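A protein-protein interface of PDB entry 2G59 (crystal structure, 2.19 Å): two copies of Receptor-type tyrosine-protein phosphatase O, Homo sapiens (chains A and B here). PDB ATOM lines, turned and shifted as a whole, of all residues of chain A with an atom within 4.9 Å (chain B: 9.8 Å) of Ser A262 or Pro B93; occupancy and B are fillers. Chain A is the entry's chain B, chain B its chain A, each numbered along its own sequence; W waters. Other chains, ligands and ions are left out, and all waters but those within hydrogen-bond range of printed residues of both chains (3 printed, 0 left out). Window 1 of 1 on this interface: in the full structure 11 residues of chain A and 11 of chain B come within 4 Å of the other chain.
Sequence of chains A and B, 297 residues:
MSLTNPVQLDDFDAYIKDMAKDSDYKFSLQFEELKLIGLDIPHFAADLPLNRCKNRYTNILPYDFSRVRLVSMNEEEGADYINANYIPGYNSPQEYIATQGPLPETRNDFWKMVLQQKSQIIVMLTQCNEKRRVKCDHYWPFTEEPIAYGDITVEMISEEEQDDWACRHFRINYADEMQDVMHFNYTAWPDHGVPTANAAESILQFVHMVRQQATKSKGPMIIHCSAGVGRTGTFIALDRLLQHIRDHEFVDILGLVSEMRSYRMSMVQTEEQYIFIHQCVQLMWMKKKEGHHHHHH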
ATOM      1  N   ILE A  37     -21.358 -14.850  -4.861  1.00  0.00           N
ATOM      2  CA  ILE A  37     -20.603 -13.719  -5.400  1.00  0.00           C
ATOM      3  C   ILE A  37     -20.933 -12.372  -4.758  1.00  0.00           C
ATOM      4  O   ILE A  37     -22.104 -12.017  -4.593  1.00  0.00           O
ATOM      5  CB  ILE A  37     -20.820 -13.575  -6.925  1.00  0.00           C
ATOM      6  CG1 ILE A  37     -20.411 -14.872  -7.639  1.00  0.00           C
ATOM      7  CG2 ILE A  37     -20.009 -12.392  -7.455  1.00  0.00           C
ATOM      8  CD1 ILE A  37     -18.930 -15.225  -7.500  1.00  0.00           C
ATOM      9  N   ILE A  41     -18.478  -7.809  -0.464  1.00  0.00           N
ATOM     10  CA  ILE A  41     -18.241  -6.482  -1.010  1.00  0.00           C
ATOM     11  C   ILE A  41     -19.070  -5.477  -0.223  1.00  0.00           C
ATOM     12  O   ILE A  41     -20.268  -5.659  -0.037  1.00  0.00           O
ATOM     13  CB  ILE A  41     -18.592  -6.427  -2.507  1.00  0.00           C
ATOM     14  CG1 ILE A  41     -17.707  -7.428  -3.262  1.00  0.00           C
ATOM     15  CG2 ILE A  41     -18.417  -4.998  -3.036  1.00  0.00           C
ATOM     16  CD1 ILE A  41     -17.901  -7.436  -4.771  1.00  0.00           C
ATOM     17  N   TYR A  63     -23.309  -1.953  -4.347  1.00  0.00           N
ATOM     18  CA  TYR A  63     -22.012  -1.979  -3.690  1.00  0.00           C
ATOM     19  C   TYR A  63     -21.480  -0.551  -3.666  1.00  0.00           C
ATOM     20  O   TYR A  63     -21.785   0.234  -4.563  1.00  0.00           O
ATOM     21  CB  TYR A  63     -21.031  -2.849  -4.467  1.00  0.00           C
ATOM     22  CG  TYR A  63     -21.498  -4.269  -4.659  1.00  0.00           C
ATOM     23  CD1 TYR A  63     -21.956  -5.022  -3.577  1.00  0.00           C
ATOM     24  CD2 TYR A  63     -21.467  -4.867  -5.922  1.00  0.00           C
ATOM     25  CE1 TYR A  63     -22.376  -6.341  -3.745  1.00  0.00           C
ATOM     26  CE2 TYR A  63     -21.881  -6.184  -6.100  1.00  0.00           C
ATOM     27  CZ  TYR A  63     -22.335  -6.919  -5.007  1.00  0.00           C
ATOM     28  OH  TYR A  63     -22.731  -8.232  -5.171  1.00  0.00           O
ATOM     29  N   PHE A  65     -18.354   0.486  -4.143  1.00  0.00           N
ATOM     30  CA  PHE A  65     -17.355   0.757  -5.178  1.00  0.00           C
ATOM     31  C   PHE A  65     -17.897   1.041  -6.579  1.00  0.00           C
ATOM     32  O   PHE A  65     -17.324   1.854  -7.311  1.00  0.00           O
ATOM     33  CB  PHE A  65     -16.334  -0.391  -5.241  1.00  0.00           C
ATOM     34  CG  PHE A  65     -16.673  -1.468  -6.243  1.00  0.00           C
ATOM     35  CD1 PHE A  65     -16.217  -1.384  -7.554  1.00  0.00           C
ATOM     36  CD2 PHE A  65     -17.441  -2.569  -5.872  1.00  0.00           C
ATOM     37  CE1 PHE A  65     -16.517  -2.380  -8.485  1.00  0.00           C
ATOM     38  CE2 PHE A  65     -17.750  -3.572  -6.796  1.00  0.00           C
ATOM     39  CZ  PHE A  65     -17.284  -3.475  -8.103  1.00  0.00           C
ATOM     40  N   SER A 258     -21.436 -14.070 -13.201  1.00  0.00           N
ATOM     41  CA  SER A 258     -20.566 -13.911 -12.043  1.00  0.00           C
ATOM     42  C   SER A 258     -20.011 -12.482 -12.071  1.00  0.00           C
ATOM     43  O   SER A 258     -19.992 -11.785 -11.051  1.00  0.00           O
ATOM     44  CB  SER A 258     -19.407 -14.910 -12.104  1.00  0.00           C
ATOM     45  OG  SER A 258     -18.484 -14.696 -11.050  1.00  0.00           O
ATOM     46  N   GLU A 259     -19.565 -12.042 -13.248  1.00  0.00           N
ATOM     47  CA  GLU A 259     -19.028 -10.695 -13.375  1.00  0.00           C
ATOM     48  C   GLU A 259     -20.070  -9.659 -12.961  1.00  0.00           C
ATOM     49  O   GLU A 259     -19.782  -8.785 -12.145  1.00  0.00           O
ATOM     50  CB  GLU A 259     -18.576 -10.405 -14.807  1.00  0.00           C
ATOM     51  CG  GLU A 259     -17.847  -9.060 -14.925  1.00  0.00           C
ATOM     52  CD  GLU A 259     -17.362  -8.762 -16.336  1.00  0.00           C
ATOM     53  OE1 GLU A 259     -18.184  -8.343 -17.174  1.00  0.00           O
ATOM     54  OE2 GLU A 259     -16.156  -8.948 -16.603  1.00  0.00           O
ATOM     55  N   MET A 260     -21.281  -9.752 -13.509  1.00  0.00           N
ATOM     56  CA  MET A 260     -22.312  -8.782 -13.149  1.00  0.00           C
ATOM     57  C   MET A 260     -22.555  -8.818 -11.635  1.00  0.00           C
ATOM     58  O   MET A 260     -22.757  -7.774 -11.014  1.00  0.00           O
ATOM     59  CB  MET A 260     -23.619  -9.054 -13.906  1.00  0.00           C
ATOM     60  CG  MET A 260     -23.485  -8.996 -15.432  1.00  0.00           C
ATOM     61  SD  MET A 260     -25.095  -8.988 -16.268  1.00  0.00           S
ATOM     62  CE  MET A 260     -25.434 -10.725 -16.339  1.00  0.00           C
ATOM     63  N   ARG A 261     -22.528 -10.013 -11.040  1.00  0.00           N
ATOM     64  CA  ARG A 261     -22.735 -10.138  -9.593  1.00  0.00           C
ATOM     65  C   ARG A 261     -21.675  -9.360  -8.809  1.00  0.00           C
ATOM     66  O   ARG A 261     -21.924  -8.919  -7.691  1.00  0.00           O
ATOM     67  CB  ARG A 261     -22.696 -11.604  -9.147  1.00  0.00           C
ATOM     68  CG  ARG A 261     -23.859 -12.470  -9.608  1.00  0.00           C
ATOM     69  CD  ARG A 261     -25.170 -11.914  -9.122  1.00  0.00           C
ATOM     70  NE  ARG A 261     -26.316 -12.764  -9.444  1.00  0.00           N
ATOM     71  CZ  ARG A 261     -26.786 -13.727  -8.658  1.00  0.00           C
ATOM     72  NH1 ARG A 261     -26.207 -13.984  -7.492  1.00  0.00           N
ATOM     73  NH2 ARG A 261     -27.868 -14.403  -9.018  1.00  0.00           N
ATOM     74  N   SER A 262     -20.493  -9.189  -9.394  1.00  0.00           N
ATOM     75  CA  SER A 262     -19.425  -8.456  -8.719  1.00  0.00           C
ATOM     76  C   SER A 262     -19.608  -6.938  -8.786  1.00  0.00           C
ATOM     77  O   SER A 262     -18.901  -6.199  -8.104  1.00  0.00           O
ATOM     78  CB  SER A 262     -18.065  -8.822  -9.322  1.00  0.00           C
ATOM     79  OG  SER A 262     -17.806 -10.212  -9.205  1.00  0.00           O
ATOM     80  N   TYR A 263     -20.547  -6.472  -9.607  1.00  0.00           N
ATOM     81  CA  TYR A 263     -20.787  -5.035  -9.734  1.00  0.00           C
ATOM     82  C   TYR A 263     -22.126  -4.624  -9.162  1.00  0.00           C
ATOM     83  O   TYR A 263     -22.316  -3.472  -8.782  1.00  0.00           O
ATOM     84  CB  TYR A 263     -20.655  -4.603 -11.202  1.00  0.00           C
ATOM     85  CG  TYR A 263     -19.208  -4.567 -11.645  1.00  0.00           C
ATOM     86  CD1 TYR A 263     -18.474  -3.371 -11.625  1.00  0.00           C
ATOM     87  CD2 TYR A 263     -18.541  -5.743 -11.989  1.00  0.00           C
ATOM     88  CE1 TYR A 263     -17.098  -3.353 -11.933  1.00  0.00           C
ATOM     89  CE2 TYR A 263     -17.177  -5.740 -12.295  1.00  0.00           C
ATOM     90  CZ  TYR A 263     -16.460  -4.545 -12.262  1.00  0.00           C
ATOM     91  OH  TYR A 263     -15.103  -4.568 -12.544  1.00  0.00           O
ATOM     92  N   ARG A 264     -23.059  -5.569  -9.107  1.00  0.00           N
ATOM     93  CA  ARG A 264     -24.376  -5.312  -8.525  1.00  0.00           C
ATOM     94  C   ARG A 264     -24.936  -6.660  -8.089  1.00  0.00           C
ATOM     95  O   ARG A 264     -24.972  -7.612  -8.871  1.00  0.00           O
ATOM     96  CB  ARG A 264     -25.316  -4.628  -9.533  1.00  0.00           C
ATOM     97  CG  ARG A 264     -26.627  -4.132  -8.906  1.00  0.00           C
ATOM     98  CD  ARG A 264     -27.476  -3.340  -9.893  1.00  0.00           C
ATOM     99  NE  ARG A 264     -28.832  -3.089  -9.396  1.00  0.00           N
ATOM    100  CZ  ARG A 264     -29.164  -2.147  -8.513  1.00  0.00           C
ATOM    101  NH1 ARG A 264     -28.238  -1.338  -8.011  1.00  0.00           N
ATOM    102  NH2 ARG A 264     -30.428  -2.020  -8.121  1.00  0.00           N
ATOM    103  N   PHE B  65     -12.355   7.020 -14.782  1.00  0.00           N
ATOM    104  CA  PHE B  65     -13.273   6.087 -14.148  1.00  0.00           C
ATOM    105  C   PHE B  65     -12.640   5.133 -13.136  1.00  0.00           C
ATOM    106  O   PHE B  65     -13.261   4.813 -12.124  1.00  0.00           O
ATOM    107  CB  PHE B  65     -14.050   5.311 -15.223  1.00  0.00           C
ATOM    108  CG  PHE B  65     -13.454   3.983 -15.580  1.00  0.00           C
ATOM    109  CD1 PHE B  65     -13.842   2.828 -14.903  1.00  0.00           C
ATOM    110  CD2 PHE B  65     -12.496   3.884 -16.585  1.00  0.00           C
ATOM    111  CE1 PHE B  65     -13.285   1.597 -15.221  1.00  0.00           C
ATOM    112  CE2 PHE B  65     -11.935   2.659 -16.910  1.00  0.00           C
ATOM    113  CZ  PHE B  65     -12.330   1.510 -16.226  1.00  0.00           C
ATOM    114  N   SER B  66     -11.409   4.697 -13.385  1.00  0.00           N
ATOM    115  CA  SER B  66     -10.762   3.756 -12.476  1.00  0.00           C
ATOM    116  C   SER B  66      -9.643   4.316 -11.600  1.00  0.00           C
ATOM    117  O   SER B  66      -9.067   3.579 -10.800  1.00  0.00           O
ATOM    118  CB  SER B  66     -10.207   2.567 -13.270  1.00  0.00           C
ATOM    119  OG  SER B  66      -9.163   2.992 -14.124  1.00  0.00           O
ATOM    120  N   ASN B  85      -4.524   3.259 -10.668  1.00  0.00           N
ATOM    121  CA  ASN B  85      -5.834   2.747 -11.065  1.00  0.00           C
ATOM    122  C   ASN B  85      -6.161   1.413 -10.414  1.00  0.00           C
ATOM    123  O   ASN B  85      -5.281   0.570 -10.210  1.00  0.00           O
ATOM    124  CB  ASN B  85      -5.899   2.535 -12.580  1.00  0.00           C
ATOM    125  CG  ASN B  85      -5.795   3.815 -13.355  1.00  0.00           C
ATOM    126  OD1 ASN B  85      -6.801   4.490 -13.616  1.00  0.00           O
ATOM    127  ND2 ASN B  85      -4.579   4.166 -13.733  1.00  0.00           N
ATOM    128  N   TYR B  86      -7.437   1.227 -10.103  1.00  0.00           N
ATOM    129  CA  TYR B  86      -7.917  -0.026  -9.540  1.00  0.00           C
ATOM    130  C   TYR B  86      -7.951  -1.002 -10.710  1.00  0.00           C
ATOM    131  O   TYR B  86      -8.426  -0.647 -11.796  1.00  0.00           O
ATOM    132  CB  TYR B  86      -9.342   0.125  -9.020  1.00  0.00           C
ATOM    133  CG  TYR B  86      -9.485   0.983  -7.803  1.00  0.00           C
ATOM    134  CD1 TYR B  86      -9.058   0.531  -6.555  1.00  0.00           C
ATOM    135  CD2 TYR B  86     -10.075   2.241  -7.886  1.00  0.00           C
ATOM    136  CE1 TYR B  86      -9.221   1.309  -5.422  1.00  0.00           C
ATOM    137  CE2 TYR B  86     -10.242   3.028  -6.760  1.00  0.00           C
ATOM    138  CZ  TYR B  86      -9.814   2.555  -5.531  1.00  0.00           C
ATOM    139  OH  TYR B  86      -9.997   3.327  -4.415  1.00  0.00           O
ATOM    140  N   ILE B  87      -7.457  -2.219 -10.492  1.00  0.00           N
ATOM    141  CA  ILE B  87      -7.454  -3.249 -11.529  1.00  0.00           C
ATOM    142  C   ILE B  87      -8.140  -4.501 -10.973  1.00  0.00           C
ATOM    143  O   ILE B  87      -7.874  -4.910  -9.840  1.00  0.00           O
ATOM    144  CB  ILE B  87      -6.012  -3.668 -11.941  1.00  0.00           C
ATOM    145  CG1 ILE B  87      -5.146  -2.441 -12.249  1.00  0.00           C
ATOM    146  CG2 ILE B  87      -6.076  -4.590 -13.148  1.00  0.00           C
ATOM    147  CD1 ILE B  87      -5.629  -1.593 -13.426  1.00  0.00           C
ATOM    148  N   PRO B  88      -9.037  -5.121 -11.757  1.00  0.00           N
ATOM    149  CA  PRO B  88      -9.714  -6.328 -11.273  1.00  0.00           C
ATOM    150  C   PRO B  88      -8.697  -7.451 -11.067  1.00  0.00           C
ATOM    151  O   PRO B  88      -7.648  -7.478 -11.721  1.00  0.00           O
ATOM    152  CB  PRO B  88     -10.691  -6.654 -12.403  1.00  0.00           C
ATOM    153  CG  PRO B  88     -11.006  -5.299 -12.968  1.00  0.00           C
ATOM    154  CD  PRO B  88      -9.635  -4.659 -13.021  1.00  0.00           C
ATOM    155  N   GLY B  89      -9.019  -8.368 -10.156  1.00  0.00           N
ATOM    156  CA  GLY B  89      -8.141  -9.493  -9.887  1.00  0.00           C
ATOM    157  C   GLY B  89      -8.894 -10.805 -10.023  1.00  0.00           C
ATOM    158  O   GLY B  89     -10.044 -10.826 -10.460  1.00  0.00           O
ATOM    159  N   TYR B  90      -8.252 -11.910  -9.663  1.00  0.00           N
ATOM    160  CA  TYR B  90      -8.913 -13.201  -9.744  1.00  0.00           C
ATOM    161  C   TYR B  90     -10.060 -13.264  -8.737  1.00  0.00           C
ATOM    162  O   TYR B  90     -11.081 -13.895  -8.999  1.00  0.00           O
ATOM    163  CB  TYR B  90      -7.921 -14.325  -9.450  1.00  0.00           C
ATOM    164  CG  TYR B  90      -8.513 -15.710  -9.578  1.00  0.00           C
ATOM    165  CD1 TYR B  90      -8.723 -16.285 -10.835  1.00  0.00           C
ATOM    166  CD2 TYR B  90      -8.870 -16.448  -8.442  1.00  0.00           C
ATOM    167  CE1 TYR B  90      -9.272 -17.556 -10.960  1.00  0.00           C
ATOM    168  CE2 TYR B  90      -9.419 -17.725  -8.553  1.00  0.00           C
ATOM    169  CZ  TYR B  90      -9.617 -18.273  -9.818  1.00  0.00           C
ATOM    170  OH  TYR B  90     -10.157 -19.534  -9.943  1.00  0.00           O
ATOM    171  N   ASN B  91      -9.897 -12.580  -7.604  1.00  0.00           N
ATOM    172  CA  ASN B  91     -10.902 -12.595  -6.535  1.00  0.00           C
ATOM    173  C   ASN B  91     -11.865 -11.409  -6.420  1.00  0.00           C
ATOM    174  O   ASN B  91     -13.005 -11.580  -5.982  1.00  0.00           O
ATOM    175  CB  ASN B  91     -10.209 -12.776  -5.182  1.00  0.00           C
ATOM    176  CG  ASN B  91      -9.162 -13.868  -5.212  1.00  0.00           C
ATOM    177  OD1 ASN B  91      -7.955 -13.598  -5.244  1.00  0.00           O
ATOM    178  ND2 ASN B  91      -9.615 -15.110  -5.218  1.00  0.00           N
ATOM    179  N   SER B  92     -11.426 -10.205  -6.773  1.00  0.00           N
ATOM    180  CA  SER B  92     -12.334  -9.066  -6.663  1.00  0.00           C
ATOM    181  C   SER B  92     -12.115  -7.958  -7.697  1.00  0.00           C
ATOM    182  O   SER B  92     -11.026  -7.823  -8.254  1.00  0.00           O
ATOM    183  CB  SER B  92     -12.272  -8.485  -5.243  1.00  0.00           C
ATOM    184  OG  SER B  92     -11.002  -7.938  -4.958  1.00  0.00           O
ATOM    185  N   PRO B  93     -13.167  -7.152  -7.960  1.00  0.00           N
ATOM    186  CA  PRO B  93     -13.199  -6.032  -8.909  1.00  0.00           C
ATOM    187  C   PRO B  93     -12.092  -4.995  -8.721  1.00  0.00           C
ATOM    188  O   PRO B  93     -11.616  -4.424  -9.695  1.00  0.00           O
ATOM    189  CB  PRO B  93     -14.576  -5.422  -8.676  1.00  0.00           C
ATOM    190  CG  PRO B  93     -15.388  -6.571  -8.251  1.00  0.00           C
ATOM    191  CD  PRO B  93     -14.475  -7.282  -7.293  1.00  0.00           C
ATOM    192  N   GLN B  94     -11.705  -4.742  -7.472  1.00  0.00           N
ATOM    193  CA  GLN B  94     -10.660  -3.764  -7.176  1.00  0.00           C
ATOM    194  C   GLN B  94      -9.574  -4.422  -6.333  1.00  0.00           C
ATOM    195  O   GLN B  94      -9.079  -3.848  -5.362  1.00  0.00           O
ATOM    196  CB  GLN B  94     -11.250  -2.554  -6.427  1.00  0.00           C
ATOM    197  CG  GLN B  94     -12.411  -1.887  -7.162  1.00  0.00           C
ATOM    198  CD  GLN B  94     -12.778  -0.516  -6.612  1.00  0.00           C
ATOM    199  OE1 GLN B  94     -12.864  -0.316  -5.395  1.00  0.00           O
ATOM    200  NE2 GLN B  94     -13.013   0.433  -7.511  1.00  0.00           N
ATOM    201  N   GLU B  95      -9.191  -5.627  -6.730  1.00  0.00           N
ATOM    202  CA  GLU B  95      -8.184  -6.380  -6.002  1.00  0.00           C
ATOM    203  C   GLU B  95      -6.810  -5.725  -5.992  1.00  0.00           C
ATOM    204  O   GLU B  95      -6.090  -5.780  -4.987  1.00  0.00           O
ATOM    205  CB  GLU B  95      -8.078  -7.786  -6.587  1.00  0.00           C
ATOM    206  CG  GLU B  95      -7.287  -8.740  -5.740  1.00  0.00           C
ATOM    207  CD  GLU B  95      -7.521 -10.175  -6.144  1.00  0.00           C
ATOM    208  OE1 GLU B  95      -8.561 -10.452  -6.789  1.00  0.00           O
ATOM    209  OE2 GLU B  95      -6.675 -11.019  -5.803  1.00  0.00           O
ATOM    210  N   TYR B  96      -6.444  -5.117  -7.113  1.00  0.00           N
ATOM    211  CA  TYR B  96      -5.145  -4.469  -7.236  1.00  0.00           C
ATOM    212  C   TYR B  96      -5.265  -2.987  -7.481  1.00  0.00           C
ATOM    213  O   TYR B  96      -6.298  -2.481  -7.930  1.00  0.00           O
ATOM    214  CB  TYR B  96      -4.350  -5.023  -8.429  1.00  0.00           C
ATOM    215  CG  TYR B  96      -4.169  -6.514  -8.457  1.00  0.00           C
ATOM    216  CD1 TYR B  96      -3.104  -7.125  -7.797  1.00  0.00           C
ATOM    217  CD2 TYR B  96      -5.060  -7.318  -9.157  1.00  0.00           C
ATOM    218  CE1 TYR B  96      -2.936  -8.510  -7.836  1.00  0.00           C
ATOM    219  CE2 TYR B  96      -4.901  -8.693  -9.202  1.00  0.00           C
ATOM    220  CZ  TYR B  96      -3.839  -9.284  -8.544  1.00  0.00           C
ATOM    221  OH  TYR B  96      -3.690 -10.651  -8.602  1.00  0.00           O
ATOM    222  N   ILE B  97      -4.177  -2.302  -7.182  1.00  0.00           N
ATOM    223  CA  ILE B  97      -4.061  -0.892  -7.457  1.00  0.00           C
ATOM    224  C   ILE B  97      -2.734  -0.849  -8.201  1.00  0.00           C
ATOM    225  O   ILE B  97      -1.689  -1.203  -7.650  1.00  0.00           O
ATOM    226  CB  ILE B  97      -3.979  -0.023  -6.199  1.00  0.00           C
ATOM    227  CG1 ILE B  97      -5.358   0.091  -5.546  1.00  0.00           C
ATOM    228  CG2 ILE B  97      -3.493   1.373  -6.583  1.00  0.00           C
ATOM    229  CD1 ILE B  97      -5.367   0.940  -4.288  1.00  0.00           C
ATOM    230  N   ALA B  98      -2.794  -0.483  -9.478  1.00  0.00           N
ATOM    231  CA  ALA B  98      -1.591  -0.382 -10.291  1.00  0.00           C
ATOM    232  C   ALA B  98      -1.218   1.089 -10.258  1.00  0.00           C
ATOM    233  O   ALA B  98      -2.052   1.946 -10.514  1.00  0.00           O
ATOM    234  CB  ALA B  98      -1.881  -0.824 -11.712  1.00  0.00           C
ATOM    235  N   PRO B 220      -6.797  -3.692  -0.894  1.00  0.00           N
ATOM    236  CA  PRO B 220      -6.206  -3.810  -2.230  1.00  0.00           C
ATOM    237  C   PRO B 220      -4.690  -4.000  -2.193  1.00  0.00           C
ATOM    238  O   PRO B 220      -4.006  -3.466  -1.320  1.00  0.00           O
ATOM    239  CB  PRO B 220      -6.609  -2.496  -2.895  1.00  0.00           C
ATOM    240  CG  PRO B 220      -6.607  -1.540  -1.752  1.00  0.00           C
ATOM    241  CD  PRO B 220      -7.304  -2.326  -0.665  1.00  0.00           C
ATOM    242  N   MET B 221      -4.175  -4.771  -3.141  1.00  0.00           N
ATOM    243  CA  MET B 221      -2.742  -5.012  -3.232  1.00  0.00           C
ATOM    244  C   MET B 221      -2.162  -3.972  -4.189  1.00  0.00           C
ATOM    245  O   MET B 221      -2.508  -3.937  -5.372  1.00  0.00           O
ATOM    246  CB  MET B 221      -2.466  -6.424  -3.764  1.00  0.00           C
ATOM    247  CG  MET B 221      -0.983  -6.808  -3.756  1.00  0.00           C
ATOM    248  SD  MET B 221      -0.625  -8.374  -4.596  1.00  0.00           S
ATOM    249  CE  MET B 221      -1.555  -9.516  -3.541  1.00  0.00           C
ATOM    250  N   ILE B 236       0.650  -8.710 -12.436  1.00  0.00           N
ATOM    251  CA  ILE B 236      -0.762  -8.919 -12.140  1.00  0.00           C
ATOM    252  C   ILE B 236      -1.326 -10.068 -12.964  1.00  0.00           C
ATOM    253  O   ILE B 236      -2.101 -10.885 -12.467  1.00  0.00           O
ATOM    254  CB  ILE B 236      -1.568  -7.623 -12.385  1.00  0.00           C
ATOM    255  CG1 ILE B 236      -1.245  -6.610 -11.277  1.00  0.00           C
ATOM    256  CG2 ILE B 236      -3.065  -7.927 -12.434  1.00  0.00           C
ATOM    257  CD1 ILE B 236      -1.965  -5.288 -11.414  1.00  0.00           C
ATOM    258  N   ARG B 240      -2.793 -13.429 -11.206  1.00  0.00           N
ATOM    259  CA  ARG B 240      -4.133 -13.885 -11.535  1.00  0.00           C
ATOM    260  C   ARG B 240      -4.130 -15.253 -12.218  1.00  0.00           C
ATOM    261  O   ARG B 240      -4.944 -16.111 -11.886  1.00  0.00           O
ATOM    262  CB  ARG B 240      -4.834 -12.853 -12.424  1.00  0.00           C
ATOM    263  CG  ARG B 240      -5.217 -11.568 -11.675  1.00  0.00           C
ATOM    264  CD  ARG B 240      -5.849 -10.513 -12.574  1.00  0.00           C
ATOM    265  NE  ARG B 240      -6.987 -11.026 -13.326  1.00  0.00           N
ATOM    266  CZ  ARG B 240      -7.823 -10.271 -14.033  1.00  0.00           C
ATOM    267  NH1 ARG B 240      -7.658  -8.953 -14.082  1.00  0.00           N
ATOM    268  NH2 ARG B 240      -8.813 -10.834 -14.713  1.00  0.00           N
ATOM    269  N   GLU B 259      -8.548  -6.876 -20.610  1.00  0.00           N
ATOM    270  CA  GLU B 259      -9.247  -6.355 -19.440  1.00  0.00           C
ATOM    271  C   GLU B 259      -8.404  -5.351 -18.650  1.00  0.00           C
ATOM    272  O   GLU B 259      -8.890  -4.274 -18.284  1.00  0.00           O
ATOM    273  CB  GLU B 259      -9.664  -7.500 -18.510  1.00  0.00           C
ATOM    274  CG  GLU B 259     -10.498  -7.039 -17.317  1.00  0.00           C
ATOM    275  CD  GLU B 259     -10.948  -8.184 -16.427  1.00  0.00           C
ATOM    276  OE1 GLU B 259     -10.148  -8.664 -15.600  1.00  0.00           O
ATOM    277  OE2 GLU B 259     -12.109  -8.612 -16.567  1.00  0.00           O
ATOM    278  N   MET B 260      -7.148  -5.695 -18.383  1.00  0.00           N
ATOM    279  CA  MET B 260      -6.281  -4.797 -17.623  1.00  0.00           C
ATOM    280  C   MET B 260      -6.142  -3.444 -18.324  1.00  0.00           C
ATOM    281  O   MET B 260      -6.115  -2.404 -17.682  1.00  0.00           O
ATOM    282  CB  MET B 260      -4.891  -5.421 -17.425  1.00  0.00           C
ATOM    283  CG  MET B 260      -4.879  -6.715 -16.613  1.00  0.00           C
ATOM    284  SD  MET B 260      -3.210  -7.135 -16.014  1.00  0.00           S
ATOM    285  CE  MET B 260      -2.500  -7.911 -17.454  1.00  0.00           C
ATOM    286  N   TYR B 263      -8.635  -0.808 -17.716  1.00  0.00           N
ATOM    287  CA  TYR B 263      -8.590  -0.204 -16.383  1.00  0.00           C
ATOM    288  C   TYR B 263      -7.371   0.694 -16.214  1.00  0.00           C
ATOM    289  O   TYR B 263      -7.390   1.633 -15.423  1.00  0.00           O
ATOM    290  CB  TYR B 263      -8.651  -1.293 -15.303  1.00  0.00           C
ATOM    291  CG  TYR B 263     -10.055  -1.819 -15.159  1.00  0.00           C
ATOM    292  CD1 TYR B 263     -10.929  -1.280 -14.211  1.00  0.00           C
ATOM    293  CD2 TYR B 263     -10.553  -2.769 -16.050  1.00  0.00           C
ATOM    294  CE1 TYR B 263     -12.266  -1.665 -14.164  1.00  0.00           C
ATOM    295  CE2 TYR B 263     -11.892  -3.162 -16.009  1.00  0.00           C
ATOM    296  CZ  TYR B 263     -12.739  -2.600 -15.065  1.00  0.00           C
ATOM    297  OH  TYR B 263     -14.064  -2.958 -15.044  1.00  0.00           O
HETATM  298  O   HOH W   1     -14.949   2.736  -6.559  1.00  0.00           O
HETATM  299  O   HOH W   2     -13.683  -2.645 -10.840  1.00  0.00           O
HETATM  300  O   HOH W   3     -14.117  -7.253 -15.442  1.00  0.00           O
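Hydrophobic or aromatic side chains of chain A within 4 Å of the printed part of chain B: Phe A65 and Tyr A263.
Of the 23 printed residues of chain B, 3 touch a printed residue of chain A.
Hydrophobic or aromatic side chains of chain B within 4 Å of the printed part of chain A: Pro B93 and Tyr B263.
Ser A262 touches just one residue of chain B: Pro B93.
Of the printed residues of chain A, Pro B93 touches Phe A65 (3.4 Å), Ser A262 (3.5 Å) and Tyr A263 (3.996 Å).
Of the printed residues of chain B, Phe A65 touches Pro B93 (3.4 Å) and Gln B94 (3.5 Å).
Of the printed residues of chain A, Gln B94 touches Phe A65.
The nearest residue of chain B that does not touch Ser A262 is Asn B91 (5.9 Å).
The nearest printed residue of chain B that does not touch Phe A65 is Ser B92 (6.9 Å).
Water W1 bridges O of Phe A65 (2.6 Å) and NE2 of Gln B94 (3.2 Å).
Water W3 bridges the side-chain carboxylate (OE2) of Glu B259 and the side-chain carboxylate (OE2) of Glu A259.
Water W2 bridges OH of Tyr A263 (2.9 Å) and O of Pro B93 (3.0 Å).
The side-chain hydroxyl (OH) of Tyr A263 is in hydrogen-bond range of the side-chain hydroxyl (OH) of Tyr B263 (3.1 Å).
Tyr B263 touches its own counterpart, Tyr A263.
Of the 5 pairs that touch across the chains among the printed residues, 1 has its exchanged pair printed and touching as well.
Pro B93 touches Phe A65.
OE1 of Gln B94 touches CB of Phe A65, at 3.5 Å.
Pro B93 touches Ser A262.
Tyr A263 touches Pro B93 (OH to CB, 3.996 Å).
OG of Ser B66 is in hydrogen-bond range of O of Tyr B263 (2.6 Å).
O of Tyr B263 sits close to OD1 of Asn B85 (3.4 Å).
The backbone carbonyl oxygen (O) of Ser A258 lies within hydrogen-bond range of the side-chain hydroxyl (OG) of Ser A262, 3.3 Å away.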
